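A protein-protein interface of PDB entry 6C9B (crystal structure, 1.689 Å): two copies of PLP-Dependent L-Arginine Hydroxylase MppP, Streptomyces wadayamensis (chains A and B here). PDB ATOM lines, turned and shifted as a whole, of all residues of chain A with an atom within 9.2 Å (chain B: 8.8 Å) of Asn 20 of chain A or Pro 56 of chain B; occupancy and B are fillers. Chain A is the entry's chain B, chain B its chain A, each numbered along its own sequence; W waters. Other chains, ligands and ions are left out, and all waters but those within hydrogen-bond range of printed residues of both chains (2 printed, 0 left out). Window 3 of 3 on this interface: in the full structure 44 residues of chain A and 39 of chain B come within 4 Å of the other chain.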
ATOM      1  N   TRP A  14      -3.358   6.981  31.659  1.00  0.00           N
ATOM      2  CA  TRP A  14      -3.704   6.298  32.909  1.00  0.00           C
ATOM      3  C   TRP A  14      -4.643   5.128  32.653  1.00  0.00           C
ATOM      4  O   TRP A  14      -4.577   4.105  33.350  1.00  0.00           O
ATOM      5  CB  TRP A  14      -4.375   7.258  33.887  1.00  0.00           C
ATOM      6  CG  TRP A  14      -3.468   8.240  34.524  1.00  0.00           C
ATOM      7  CD1 TRP A  14      -3.317   9.559  34.194  1.00  0.00           C
ATOM      8  CD2 TRP A  14      -2.593   7.999  35.631  1.00  0.00           C
ATOM      9  NE1 TRP A  14      -2.395  10.149  35.025  1.00  0.00           N
ATOM     10  CE2 TRP A  14      -1.934   9.213  35.915  1.00  0.00           C
ATOM     11  CE3 TRP A  14      -2.302   6.874  36.407  1.00  0.00           C
ATOM     12  CZ2 TRP A  14      -0.999   9.331  36.943  1.00  0.00           C
ATOM     13  CZ3 TRP A  14      -1.374   6.993  37.424  1.00  0.00           C
ATOM     14  CH2 TRP A  14      -0.733   8.212  37.684  1.00  0.00           C
ATOM     15  N   GLU A  15      -5.537   5.267  31.671  1.00  0.00           N
ATOM     16  CA  GLU A  15      -6.490   4.200  31.394  1.00  0.00           C
ATOM     17  C   GLU A  15      -5.828   2.997  30.724  1.00  0.00           C
ATOM     18  O   GLU A  15      -6.303   1.876  30.904  1.00  0.00           O
ATOM     19  CB  GLU A  15      -7.650   4.735  30.549  1.00  0.00           C
ATOM     20  CG  GLU A  15      -8.469   5.802  31.303  1.00  0.00           C
ATOM     21  CD  GLU A  15      -9.595   6.432  30.482  1.00  0.00           C
ATOM     22  OE1 GLU A  15      -9.641   6.271  29.251  1.00  0.00           O
ATOM     23  OE2 GLU A  15     -10.463   7.082  31.089  1.00  0.00           O
ATOM     24  N   TYR A  16      -4.741   3.186  29.957  1.00  0.00           N
ATOM     25  CA  TYR A  16      -4.056   2.035  29.362  1.00  0.00           C
ATOM     26  C   TYR A  16      -3.626   1.043  30.433  1.00  0.00           C
ATOM     27  O   TYR A  16      -3.617  -0.176  30.204  1.00  0.00           O
ATOM     28  CB  TYR A  16      -2.814   2.476  28.566  1.00  0.00           C
ATOM     29  CG  TYR A  16      -3.117   3.265  27.313  1.00  0.00           C
ATOM     30  CD1 TYR A  16      -4.203   2.942  26.522  1.00  0.00           C
ATOM     31  CD2 TYR A  16      -2.312   4.334  26.922  1.00  0.00           C
ATOM     32  CE1 TYR A  16      -4.498   3.656  25.366  1.00  0.00           C
ATOM     33  CE2 TYR A  16      -2.601   5.068  25.769  1.00  0.00           C
ATOM     34  CZ  TYR A  16      -3.702   4.726  24.998  1.00  0.00           C
ATOM     35  OH  TYR A  16      -4.025   5.442  23.855  1.00  0.00           O
ATOM     36  N   LEU A  17      -3.227   1.557  31.597  1.00  0.00           N
ATOM     37  CA  LEU A  17      -2.657   0.721  32.648  1.00  0.00           C
ATOM     38  C   LEU A  17      -3.677  -0.259  33.205  1.00  0.00           C
ATOM     39  O   LEU A  17      -3.291  -1.283  33.793  1.00  0.00           O
ATOM     40  CB  LEU A  17      -2.125   1.606  33.777  1.00  0.00           C
ATOM     41  CG  LEU A  17      -1.036   2.623  33.422  1.00  0.00           C
ATOM     42  CD1 LEU A  17      -0.826   3.576  34.587  1.00  0.00           C
ATOM     43  CD2 LEU A  17       0.259   1.927  33.062  1.00  0.00           C
ATOM     44  N   ALA A  18      -4.964   0.033  33.021  1.00  0.00           N
ATOM     45  CA  ALA A  18      -6.052  -0.747  33.604  1.00  0.00           C
ATOM     46  C   ALA A  18      -6.689  -1.737  32.637  1.00  0.00           C
ATOM     47  O   ALA A  18      -7.384  -2.650  33.090  1.00  0.00           O
ATOM     48  CB  ALA A  18      -7.158   0.190  34.117  1.00  0.00           C
ATOM     49  N   LEU A  19      -6.456  -1.590  31.328  1.00  0.00           N
ATOM     50  CA  LEU A  19      -7.283  -2.261  30.325  1.00  0.00           C
ATOM     51  C   LEU A  19      -7.292  -3.771  30.476  1.00  0.00           C
ATOM     52  O   LEU A  19      -8.258  -4.425  30.065  1.00  0.00           O
ATOM     53  CB  LEU A  19      -6.794  -1.919  28.923  1.00  0.00           C
ATOM     54  CG  LEU A  19      -7.310  -0.651  28.265  1.00  0.00           C
ATOM     55  CD1 LEU A  19      -6.725  -0.579  26.863  1.00  0.00           C
ATOM     56  CD2 LEU A  19      -8.828  -0.634  28.226  1.00  0.00           C
ATOM     57  N   ASN A  20      -6.217  -4.347  31.010  1.00  0.00           N
ATOM     58  CA  ASN A  20      -6.064  -5.794  31.052  1.00  0.00           C
ATOM     59  C   ASN A  20      -6.198  -6.348  32.465  1.00  0.00           C
ATOM     60  O   ASN A  20      -5.887  -7.522  32.700  1.00  0.00           O
ATOM     61  CB  ASN A  20      -4.725  -6.173  30.423  1.00  0.00           C
ATOM     62  CG  ASN A  20      -4.629  -5.684  28.994  1.00  0.00           C
ATOM     63  OD1 ASN A  20      -5.298  -6.219  28.115  1.00  0.00           O
ATOM     64  ND2 ASN A  20      -3.848  -4.633  28.765  1.00  0.00           N
ATOM     65  N   SER A  21      -6.701  -5.536  33.391  1.00  0.00           N
ATOM     66  CA  SER A  21      -6.836  -5.904  34.793  1.00  0.00           C
ATOM     67  C   SER A  21      -8.279  -6.269  35.115  1.00  0.00           C
ATOM     68  O   SER A  21      -9.225  -5.701  34.562  1.00  0.00           O
ATOM     69  CB  SER A  21      -6.376  -4.756  35.697  1.00  0.00           C
ATOM     70  OG  SER A  21      -6.949  -4.868  36.991  1.00  0.00           O
ATOM     71  N   GLU A  22      -8.438  -7.233  36.026  1.00  0.00           N
ATOM     72  CA  GLU A  22      -9.772  -7.642  36.449  1.00  0.00           C
ATOM     73  C   GLU A  22     -10.497  -6.527  37.196  1.00  0.00           C
ATOM     74  O   GLU A  22     -11.726  -6.414  37.102  1.00  0.00           O
ATOM     75  CB  GLU A  22      -9.672  -8.901  37.326  1.00  0.00           C
ATOM     76  CG  GLU A  22      -9.132 -10.136  36.583  1.00  0.00           C
ATOM     77  CD  GLU A  22      -8.523 -11.185  37.517  1.00  0.00           C
ATOM     78  OE1 GLU A  22      -8.861 -11.190  38.720  1.00  0.00           O
ATOM     79  OE2 GLU A  22      -7.704 -12.006  37.043  1.00  0.00           O
ATOM     80  N   LEU A  23      -9.765  -5.696  37.938  1.00  0.00           N
ATOM     81  CA  LEU A  23     -10.394  -4.646  38.720  1.00  0.00           C
ATOM     82  C   LEU A  23     -10.086  -3.300  38.095  1.00  0.00           C
ATOM     83  O   LEU A  23      -9.577  -2.389  38.754  1.00  0.00           O
ATOM     84  CB  LEU A  23      -9.943  -4.711  40.178  1.00  0.00           C
ATOM     85  CG  LEU A  23     -10.285  -6.063  40.815  1.00  0.00           C
ATOM     86  CD1 LEU A  23      -9.731  -6.142  42.212  1.00  0.00           C
ATOM     87  CD2 LEU A  23     -11.785  -6.292  40.874  1.00  0.00           C
ATOM     88  N   ASN A  24     -10.387  -3.192  36.807  1.00  0.00           N
ATOM     89  CA  ASN A  24     -10.330  -1.919  36.092  1.00  0.00           C
ATOM     90  C   ASN A  24     -11.583  -1.134  36.469  1.00  0.00           C
ATOM     91  O   ASN A  24     -12.701  -1.560  36.170  1.00  0.00           O
ATOM     92  CB  ASN A  24     -10.217  -2.192  34.591  1.00  0.00           C
ATOM     93  CG  ASN A  24     -10.587  -0.992  33.709  1.00  0.00           C
ATOM     94  OD1 ASN A  24     -10.789   0.128  34.181  1.00  0.00           O
ATOM     95  ND2 ASN A  24     -10.696  -1.247  32.403  1.00  0.00           N
ATOM     96  N   ILE A  25     -11.411  -0.028  37.206  1.00  0.00           N
ATOM     97  CA  ILE A  25     -12.506   0.920  37.449  1.00  0.00           C
ATOM     98  C   ILE A  25     -12.054   2.298  36.978  1.00  0.00           C
ATOM     99  O   ILE A  25     -12.404   3.335  37.562  1.00  0.00           O
ATOM    100  CB  ILE A  25     -12.951   0.927  38.926  1.00  0.00           C
ATOM    101  CG1 ILE A  25     -11.740   1.102  39.863  1.00  0.00           C
ATOM    102  CG2 ILE A  25     -13.720  -0.354  39.231  1.00  0.00           C
ATOM    103  CD1 ILE A  25     -12.121   1.479  41.290  1.00  0.00           C
ATOM    104  N   ALA A  26     -11.301   2.314  35.884  1.00  0.00           N
ATOM    105  CA  ALA A  26     -10.687   3.522  35.364  1.00  0.00           C
ATOM    106  C   ALA A  26     -11.450   4.072  34.161  1.00  0.00           C
ATOM    107  O   ALA A  26     -12.144   5.088  34.281  1.00  0.00           O
ATOM    108  CB  ALA A  26      -9.227   3.277  34.970  1.00  0.00           C
ATOM    109  N   ASP A  27     -11.314   3.448  32.991  1.00  0.00           N
ATOM    110  CA  ASP A  27     -11.918   4.067  31.820  1.00  0.00           C
ATOM    111  C   ASP A  27     -13.439   4.001  31.921  1.00  0.00           C
ATOM    112  O   ASP A  27     -14.020   3.147  32.600  1.00  0.00           O
ATOM    113  CB  ASP A  27     -11.455   3.411  30.524  1.00  0.00           C
ATOM    114  CG  ASP A  27     -11.926   1.999  30.415  1.00  0.00           C
ATOM    115  OD1 ASP A  27     -13.154   1.798  30.260  1.00  0.00           O
ATOM    116  OD2 ASP A  27     -11.059   1.106  30.476  1.00  0.00           O
ATOM    117  N   ARG A  31     -18.542  -1.916  30.550  1.00  0.00           N
ATOM    118  CA  ARG A  31     -17.983  -3.256  30.600  1.00  0.00           C
ATOM    119  C   ARG A  31     -18.803  -4.204  31.482  1.00  0.00           C
ATOM    120  O   ARG A  31     -18.339  -5.314  31.772  1.00  0.00           O
ATOM    121  CB  ARG A  31     -16.513  -3.171  31.058  1.00  0.00           C
ATOM    122  CG  ARG A  31     -15.652  -2.191  30.180  1.00  0.00           C
ATOM    123  CD  ARG A  31     -14.171  -2.132  30.565  1.00  0.00           C
ATOM    124  NE  ARG A  31     -13.458  -1.105  29.786  1.00  0.00           N
ATOM    125  CZ  ARG A  31     -13.020  -1.280  28.540  1.00  0.00           C
ATOM    126  NH1 ARG A  31     -13.216  -2.434  27.910  1.00  0.00           N
ATOM    127  NH2 ARG A  31     -12.383  -0.299  27.918  1.00  0.00           N
ATOM    128  N   HIS A 330      -3.838  -4.225  42.691  1.00  0.00           N
ATOM    129  CA  HIS A 330      -4.341  -4.552  41.358  1.00  0.00           C
ATOM    130  C   HIS A 330      -5.722  -3.959  41.086  1.00  0.00           C
ATOM    131  O   HIS A 330      -6.488  -4.506  40.290  1.00  0.00           O
ATOM    132  CB  HIS A 330      -4.355  -6.067  41.140  1.00  0.00           C
ATOM    133  CG  HIS A 330      -3.046  -6.723  41.450  1.00  0.00           C
ATOM    134  ND1 HIS A 330      -2.780  -7.320  42.664  1.00  0.00           N
ATOM    135  CD2 HIS A 330      -1.919  -6.854  40.712  1.00  0.00           C
ATOM    136  CE1 HIS A 330      -1.550  -7.802  42.655  1.00  0.00           C
ATOM    137  NE2 HIS A 330      -1.007  -7.534  41.481  1.00  0.00           N
ATOM    138  N   PHE A 332      -7.447  -0.471  39.608  1.00  0.00           N
ATOM    139  CA  PHE A 332      -7.053   0.668  38.775  1.00  0.00           C
ATOM    140  C   PHE A 332      -8.184   1.678  38.661  1.00  0.00           C
ATOM    141  O   PHE A 332      -9.171   1.448  37.950  1.00  0.00           O
ATOM    142  CB  PHE A 332      -6.612   0.200  37.391  1.00  0.00           C
ATOM    143  CG  PHE A 332      -5.343  -0.582  37.415  1.00  0.00           C
ATOM    144  CD1 PHE A 332      -4.120   0.061  37.323  1.00  0.00           C
ATOM    145  CD2 PHE A 332      -5.364  -1.965  37.560  1.00  0.00           C
ATOM    146  CE1 PHE A 332      -2.939  -0.661  37.355  1.00  0.00           C
ATOM    147  CE2 PHE A 332      -4.188  -2.681  37.595  1.00  0.00           C
ATOM    148  CZ  PHE A 332      -2.976  -2.030  37.497  1.00  0.00           C
ATOM    149  N   ALA B  50     -18.108 -13.344  23.056  1.00  0.00           N
ATOM    150  CA  ALA B  50     -17.829 -13.831  24.398  1.00  0.00           C
ATOM    151  C   ALA B  50     -16.338 -13.819  24.694  1.00  0.00           C
ATOM    152  O   ALA B  50     -15.919 -13.490  25.813  1.00  0.00           O
ATOM    153  CB  ALA B  50     -18.412 -15.240  24.557  1.00  0.00           C
ATOM    154  N   GLU B  51     -15.517 -14.205  23.716  1.00  0.00           N
ATOM    155  CA  GLU B  51     -14.068 -14.146  23.903  1.00  0.00           C
ATOM    156  C   GLU B  51     -13.621 -12.726  24.228  1.00  0.00           C
ATOM    157  O   GLU B  51     -12.805 -12.507  25.133  1.00  0.00           O
ATOM    158  CB  GLU B  51     -13.342 -14.638  22.651  1.00  0.00           C
ATOM    159  CG  GLU B  51     -11.834 -14.681  22.849  1.00  0.00           C
ATOM    160  CD  GLU B  51     -11.050 -15.065  21.606  1.00  0.00           C
ATOM    161  OE1 GLU B  51     -11.656 -15.454  20.592  1.00  0.00           O
ATOM    162  OE2 GLU B  51      -9.811 -14.995  21.668  1.00  0.00           O
ATOM    163  N   SER B  52     -14.190 -11.754  23.533  1.00  0.00           N
ATOM    164  CA  SER B  52     -13.780 -10.357  23.700  1.00  0.00           C
ATOM    165  C   SER B  52     -14.240  -9.779  25.030  1.00  0.00           C
ATOM    166  O   SER B  52     -13.604  -8.855  25.559  1.00  0.00           O
ATOM    167  CB  SER B  52     -14.332  -9.522  22.546  1.00  0.00           C
ATOM    168  OG  SER B  52     -13.863  -9.989  21.308  1.00  0.00           O
ATOM    169  N   GLU B  53     -15.339 -10.285  25.584  1.00  0.00           N
ATOM    170  CA  GLU B  53     -15.737  -9.890  26.926  1.00  0.00           C
ATOM    171  C   GLU B  53     -14.834 -10.495  27.981  1.00  0.00           C
ATOM    172  O   GLU B  53     -14.649  -9.900  29.048  1.00  0.00           O
ATOM    173  CB  GLU B  53     -17.174 -10.318  27.236  1.00  0.00           C
ATOM    174  CG  GLU B  53     -18.234  -9.694  26.427  1.00  0.00           C
ATOM    175  CD  GLU B  53     -19.619 -10.244  26.772  1.00  0.00           C
ATOM    176  OE1 GLU B  53     -20.476  -9.465  27.241  1.00  0.00           O
ATOM    177  OE2 GLU B  53     -19.843 -11.459  26.579  1.00  0.00           O
ATOM    178  N   GLN B  54     -14.314 -11.703  27.739  1.00  0.00           N
ATOM    179  CA  GLN B  54     -13.668 -12.446  28.799  1.00  0.00           C
ATOM    180  C   GLN B  54     -12.157 -12.293  28.843  1.00  0.00           C
ATOM    181  O   GLN B  54     -11.572 -12.441  29.920  1.00  0.00           O
ATOM    182  CB  GLN B  54     -14.003 -13.937  28.658  1.00  0.00           C
ATOM    183  CG  GLN B  54     -15.455 -14.282  28.960  1.00  0.00           C
ATOM    184  CD  GLN B  54     -15.813 -14.123  30.435  1.00  0.00           C
ATOM    185  OE1 GLN B  54     -14.968 -14.276  31.319  1.00  0.00           O
ATOM    186  NE2 GLN B  54     -17.075 -13.822  30.701  1.00  0.00           N
ATOM    187  N   ARG B  55     -11.508 -12.063  27.717  1.00  0.00           N
ATOM    188  CA  ARG B  55     -10.053 -12.084  27.687  1.00  0.00           C
ATOM    189  C   ARG B  55      -9.484 -10.667  27.728  1.00  0.00           C
ATOM    190  O   ARG B  55     -10.135  -9.717  27.291  1.00  0.00           O
ATOM    191  CB  ARG B  55      -9.540 -12.766  26.425  1.00  0.00           C
ATOM    192  CG  ARG B  55      -9.890 -14.260  26.316  1.00  0.00           C
ATOM    193  CD  ARG B  55      -9.240 -14.799  25.041  1.00  0.00           C
ATOM    194  NE  ARG B  55      -7.782 -14.842  25.175  1.00  0.00           N
ATOM    195  CZ  ARG B  55      -6.925 -14.874  24.161  1.00  0.00           C
ATOM    196  NH1 ARG B  55      -7.357 -14.877  22.900  1.00  0.00           N
ATOM    197  NH2 ARG B  55      -5.623 -14.904  24.406  1.00  0.00           N
ATOM    198  N   PRO B  56      -8.270 -10.505  28.253  1.00  0.00           N
ATOM    199  CA  PRO B  56      -7.608  -9.198  28.173  1.00  0.00           C
ATOM    200  C   PRO B  56      -7.429  -8.766  26.722  1.00  0.00           C
ATOM    201  O   PRO B  56      -6.920  -9.520  25.887  1.00  0.00           O
ATOM    202  CB  PRO B  56      -6.259  -9.440  28.862  1.00  0.00           C
ATOM    203  CG  PRO B  56      -6.437 -10.663  29.675  1.00  0.00           C
ATOM    204  CD  PRO B  56      -7.458 -11.499  28.984  1.00  0.00           C
ATOM    205  N   VAL B  57      -7.816  -7.520  26.426  1.00  0.00           N
ATOM    206  CA  VAL B  57      -7.704  -7.061  25.045  1.00  0.00           C
ATOM    207  C   VAL B  57      -6.265  -7.176  24.550  1.00  0.00           C
ATOM    208  O   VAL B  57      -6.037  -7.420  23.360  1.00  0.00           O
ATOM    209  CB  VAL B  57      -8.248  -5.622  24.887  1.00  0.00           C
ATOM    210  CG1 VAL B  57      -7.477  -4.637  25.759  1.00  0.00           C
ATOM    211  CG2 VAL B  57      -8.208  -5.196  23.416  1.00  0.00           C
ATOM    212  N   GLN B  58      -5.271  -7.000  25.432  1.00  0.00           N
ATOM    213  CA  GLN B  58      -3.881  -7.046  24.977  1.00  0.00           C
ATOM    214  C   GLN B  58      -3.530  -8.400  24.385  1.00  0.00           C
ATOM    215  O   GLN B  58      -2.735  -8.470  23.443  1.00  0.00           O
ATOM    216  CB  GLN B  58      -2.911  -6.726  26.114  1.00  0.00           C
ATOM    217  CG  GLN B  58      -1.427  -6.807  25.704  1.00  0.00           C
ATOM    218  CD  GLN B  58      -1.029  -5.719  24.716  1.00  0.00           C
ATOM    219  OE1 GLN B  58      -1.137  -4.528  25.013  1.00  0.00           O
ATOM    220  NE2 GLN B  58      -0.569  -6.124  23.533  1.00  0.00           N
ATOM    221  N   GLN B  59      -4.104  -9.487  24.922  1.00  0.00           N
ATOM    222  CA  GLN B  59      -3.827 -10.804  24.357  1.00  0.00           C
ATOM    223  C   GLN B  59      -4.457 -10.938  22.985  1.00  0.00           C
ATOM    224  O   GLN B  59      -3.834 -11.463  22.056  1.00  0.00           O
ATOM    225  CB  GLN B  59      -4.339 -11.905  25.288  1.00  0.00           C
ATOM    226  CG  GLN B  59      -3.641 -11.933  26.621  1.00  0.00           C
ATOM    227  CD  GLN B  59      -4.193 -13.012  27.543  1.00  0.00           C
ATOM    228  OE1 GLN B  59      -4.834 -13.976  27.100  1.00  0.00           O
ATOM    229  NE2 GLN B  59      -3.954 -12.847  28.834  1.00  0.00           N
ATOM    230  N   ILE B  60      -5.692 -10.463  22.833  1.00  0.00           N
ATOM    231  CA  ILE B  60      -6.350 -10.555  21.539  1.00  0.00           C
ATOM    232  C   ILE B  60      -5.599  -9.707  20.526  1.00  0.00           C
ATOM    233  O   ILE B  60      -5.399 -10.110  19.375  1.00  0.00           O
ATOM    234  CB  ILE B  60      -7.825 -10.130  21.653  1.00  0.00           C
ATOM    235  CG1 ILE B  60      -8.603 -11.063  22.618  1.00  0.00           C
ATOM    236  CG2 ILE B  60      -8.482 -10.092  20.255  1.00  0.00           C
ATOM    237  CD1 ILE B  60     -10.031 -10.655  22.895  1.00  0.00           C
ATOM    238  N   GLU B  61      -5.194  -8.510  20.935  1.00  0.00           N
ATOM    239  CA  GLU B  61      -4.474  -7.617  20.033  1.00  0.00           C
ATOM    240  C   GLU B  61      -3.137  -8.214  19.591  1.00  0.00           C
ATOM    241  O   GLU B  61      -2.787  -8.162  18.403  1.00  0.00           O
ATOM    242  CB  GLU B  61      -4.261  -6.266  20.713  1.00  0.00           C
ATOM    243  CG  GLU B  61      -3.663  -5.260  19.748  1.00  0.00           C
ATOM    244  CD  GLU B  61      -3.337  -3.927  20.380  1.00  0.00           C
ATOM    245  OE1 GLU B  61      -3.115  -3.873  21.594  1.00  0.00           O
ATOM    246  OE2 GLU B  61      -3.272  -2.939  19.641  1.00  0.00           O
ATOM    247  N   SER B  62      -2.361  -8.761  20.539  1.00  0.00           N
ATOM    248  CA  SER B  62      -1.084  -9.366  20.167  1.00  0.00           C
ATOM    249  C   SER B  62      -1.302 -10.502  19.191  1.00  0.00           C
ATOM    250  O   SER B  62      -0.506 -10.699  18.272  1.00  0.00           O
ATOM    251  CB  SER B  62      -0.344  -9.873  21.404  1.00  0.00           C
ATOM    252  OG  SER B  62       0.200  -8.774  22.110  1.00  0.00           O
ATOM    253  N   GLU B  63      -2.357 -11.296  19.406  1.00  0.00           N
ATOM    254  CA  GLU B  63      -2.632 -12.416  18.509  1.00  0.00           C
ATOM    255  C   GLU B  63      -3.044 -11.929  17.130  1.00  0.00           C
ATOM    256  O   GLU B  63      -2.668 -12.527  16.116  1.00  0.00           O
ATOM    257  CB  GLU B  63      -3.720 -13.306  19.107  1.00  0.00           C
ATOM    258  CG  GLU B  63      -3.288 -13.999  20.341  1.00  0.00           C
ATOM    259  CD  GLU B  63      -4.424 -14.729  21.047  1.00  0.00           C
ATOM    260  OE1 GLU B  63      -4.137 -15.417  22.048  1.00  0.00           O
ATOM    261  OE2 GLU B  63      -5.599 -14.612  20.620  1.00  0.00           O
ATOM    262  N   PRO B  81       4.371  -4.857  23.407  1.00  0.00           N
ATOM    263  CA  PRO B  81       3.156  -4.040  23.517  1.00  0.00           C
ATOM    264  C   PRO B  81       3.465  -2.552  23.443  1.00  0.00           C
ATOM    265  O   PRO B  81       4.446  -2.069  24.014  1.00  0.00           O
ATOM    266  CB  PRO B  81       2.585  -4.448  24.878  1.00  0.00           C
ATOM    267  CG  PRO B  81       2.995  -5.891  25.009  1.00  0.00           C
ATOM    268  CD  PRO B  81       4.360  -5.984  24.354  1.00  0.00           C
ATOM    269  N   PRO B 256     -12.086  -5.036  20.807  1.00  0.00           N
ATOM    270  CA  PRO B 256     -11.534  -6.397  20.800  1.00  0.00           C
ATOM    271  C   PRO B 256     -12.220  -7.315  19.808  1.00  0.00           C
ATOM    272  O   PRO B 256     -11.600  -8.285  19.337  1.00  0.00           O
ATOM    273  CB  PRO B 256     -11.745  -6.882  22.246  1.00  0.00           C
ATOM    274  CG  PRO B 256     -12.803  -6.007  22.818  1.00  0.00           C
ATOM    275  CD  PRO B 256     -12.567  -4.648  22.138  1.00  0.00           C
ATOM    276  N   LEU B 259     -10.463  -6.810  16.553  1.00  0.00           N
ATOM    277  CA  LEU B 259      -9.161  -7.465  16.612  1.00  0.00           C
ATOM    278  C   LEU B 259      -9.306  -8.979  16.500  1.00  0.00           C
ATOM    279  O   LEU B 259      -8.541  -9.635  15.777  1.00  0.00           O
ATOM    280  CB  LEU B 259      -8.451  -7.091  17.916  1.00  0.00           C
ATOM    281  CG  LEU B 259      -8.007  -5.618  18.004  1.00  0.00           C
ATOM    282  CD1 LEU B 259      -7.613  -5.271  19.422  1.00  0.00           C
ATOM    283  CD2 LEU B 259      -6.851  -5.352  17.027  1.00  0.00           C
ATOM    284  N   ARG B 263      -7.834 -11.367  13.546  1.00  0.00           N
ATOM    285  CA  ARG B 263      -7.087 -12.582  13.838  1.00  0.00           C
ATOM    286  C   ARG B 263      -7.644 -13.765  13.055  1.00  0.00           C
ATOM    287  O   ARG B 263      -6.898 -14.505  12.393  1.00  0.00           O
ATOM    288  CB  ARG B 263      -7.141 -12.853  15.344  1.00  0.00           C
ATOM    289  CG  ARG B 263      -6.302 -14.037  15.781  1.00  0.00           C
ATOM    290  CD  ARG B 263      -6.650 -14.443  17.196  1.00  0.00           C
ATOM    291  NE  ARG B 263      -8.021 -14.960  17.274  1.00  0.00           N
ATOM    292  CZ  ARG B 263      -8.793 -14.882  18.357  1.00  0.00           C
ATOM    293  NH1 ARG B 263      -8.335 -14.341  19.482  1.00  0.00           N
ATOM    294  NH2 ARG B 263     -10.025 -15.375  18.320  1.00  0.00           N
HETATM  295  O   HOH W   1      -3.420  -3.241  26.147  1.00  0.00           O
HETATM  296  O   HOH W   2      -9.221  -6.245  28.550  1.00  0.00           O
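Among the printed residues, pairs that only touch across the chains: Asn 20 of chain A with Pro 56 of chain B.
No position is printed for both chains.
Water W2 lies within hydrogen-bond range of O of Leu 19 of chain A and N of Val 57 of chain B. Water W1 lies within hydrogen-bond range of OE1 of Gln 58 of chain B (2.9 Å) and ND2 of Asn 20 of chain A (3.0 Å).
Printed residues of chain B that touch a printed residue of chain A: Pro 56, Val 57 and Gln 58. Among the printed residues, 3 pairs touch across the chains.
The side-chain hydroxyl (OG) of Ser 62 of chain B is in hydrogen-bond range of the side-chain amide nitrogen (NE2) of Gln 58 of chain B, at 3.1 Å.
Of chain B, only Pro 56, Val 57 and Gln 58 come within 4 Å of Asn 20 of chain A. Of chain A, only Asn 20 (3.4 Å) comes within 4 Å of Pro 56 of chain B. Of chain A, only Asn 20 comes within 4 Å of Val 57 of chain B. Of the printed residues of chain A, Gln 58 of chain B touches Asn 20 (2.8 Å). Leu 23 of chain A touches none of the printed residues of chain B. The nearest residue of chain B that does not touch Asn 20 of chain A is Gln 59 of chain B (4.7 Å).
OD1 of Asn 20 of chain A is in hydrogen-bond range of N of Gln 58 of chain B, at 2.8 Å. N of Val 57 of chain B lies within hydrogen-bond range of OD1 of Asn 20 of chain A, at 3.3 Å.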
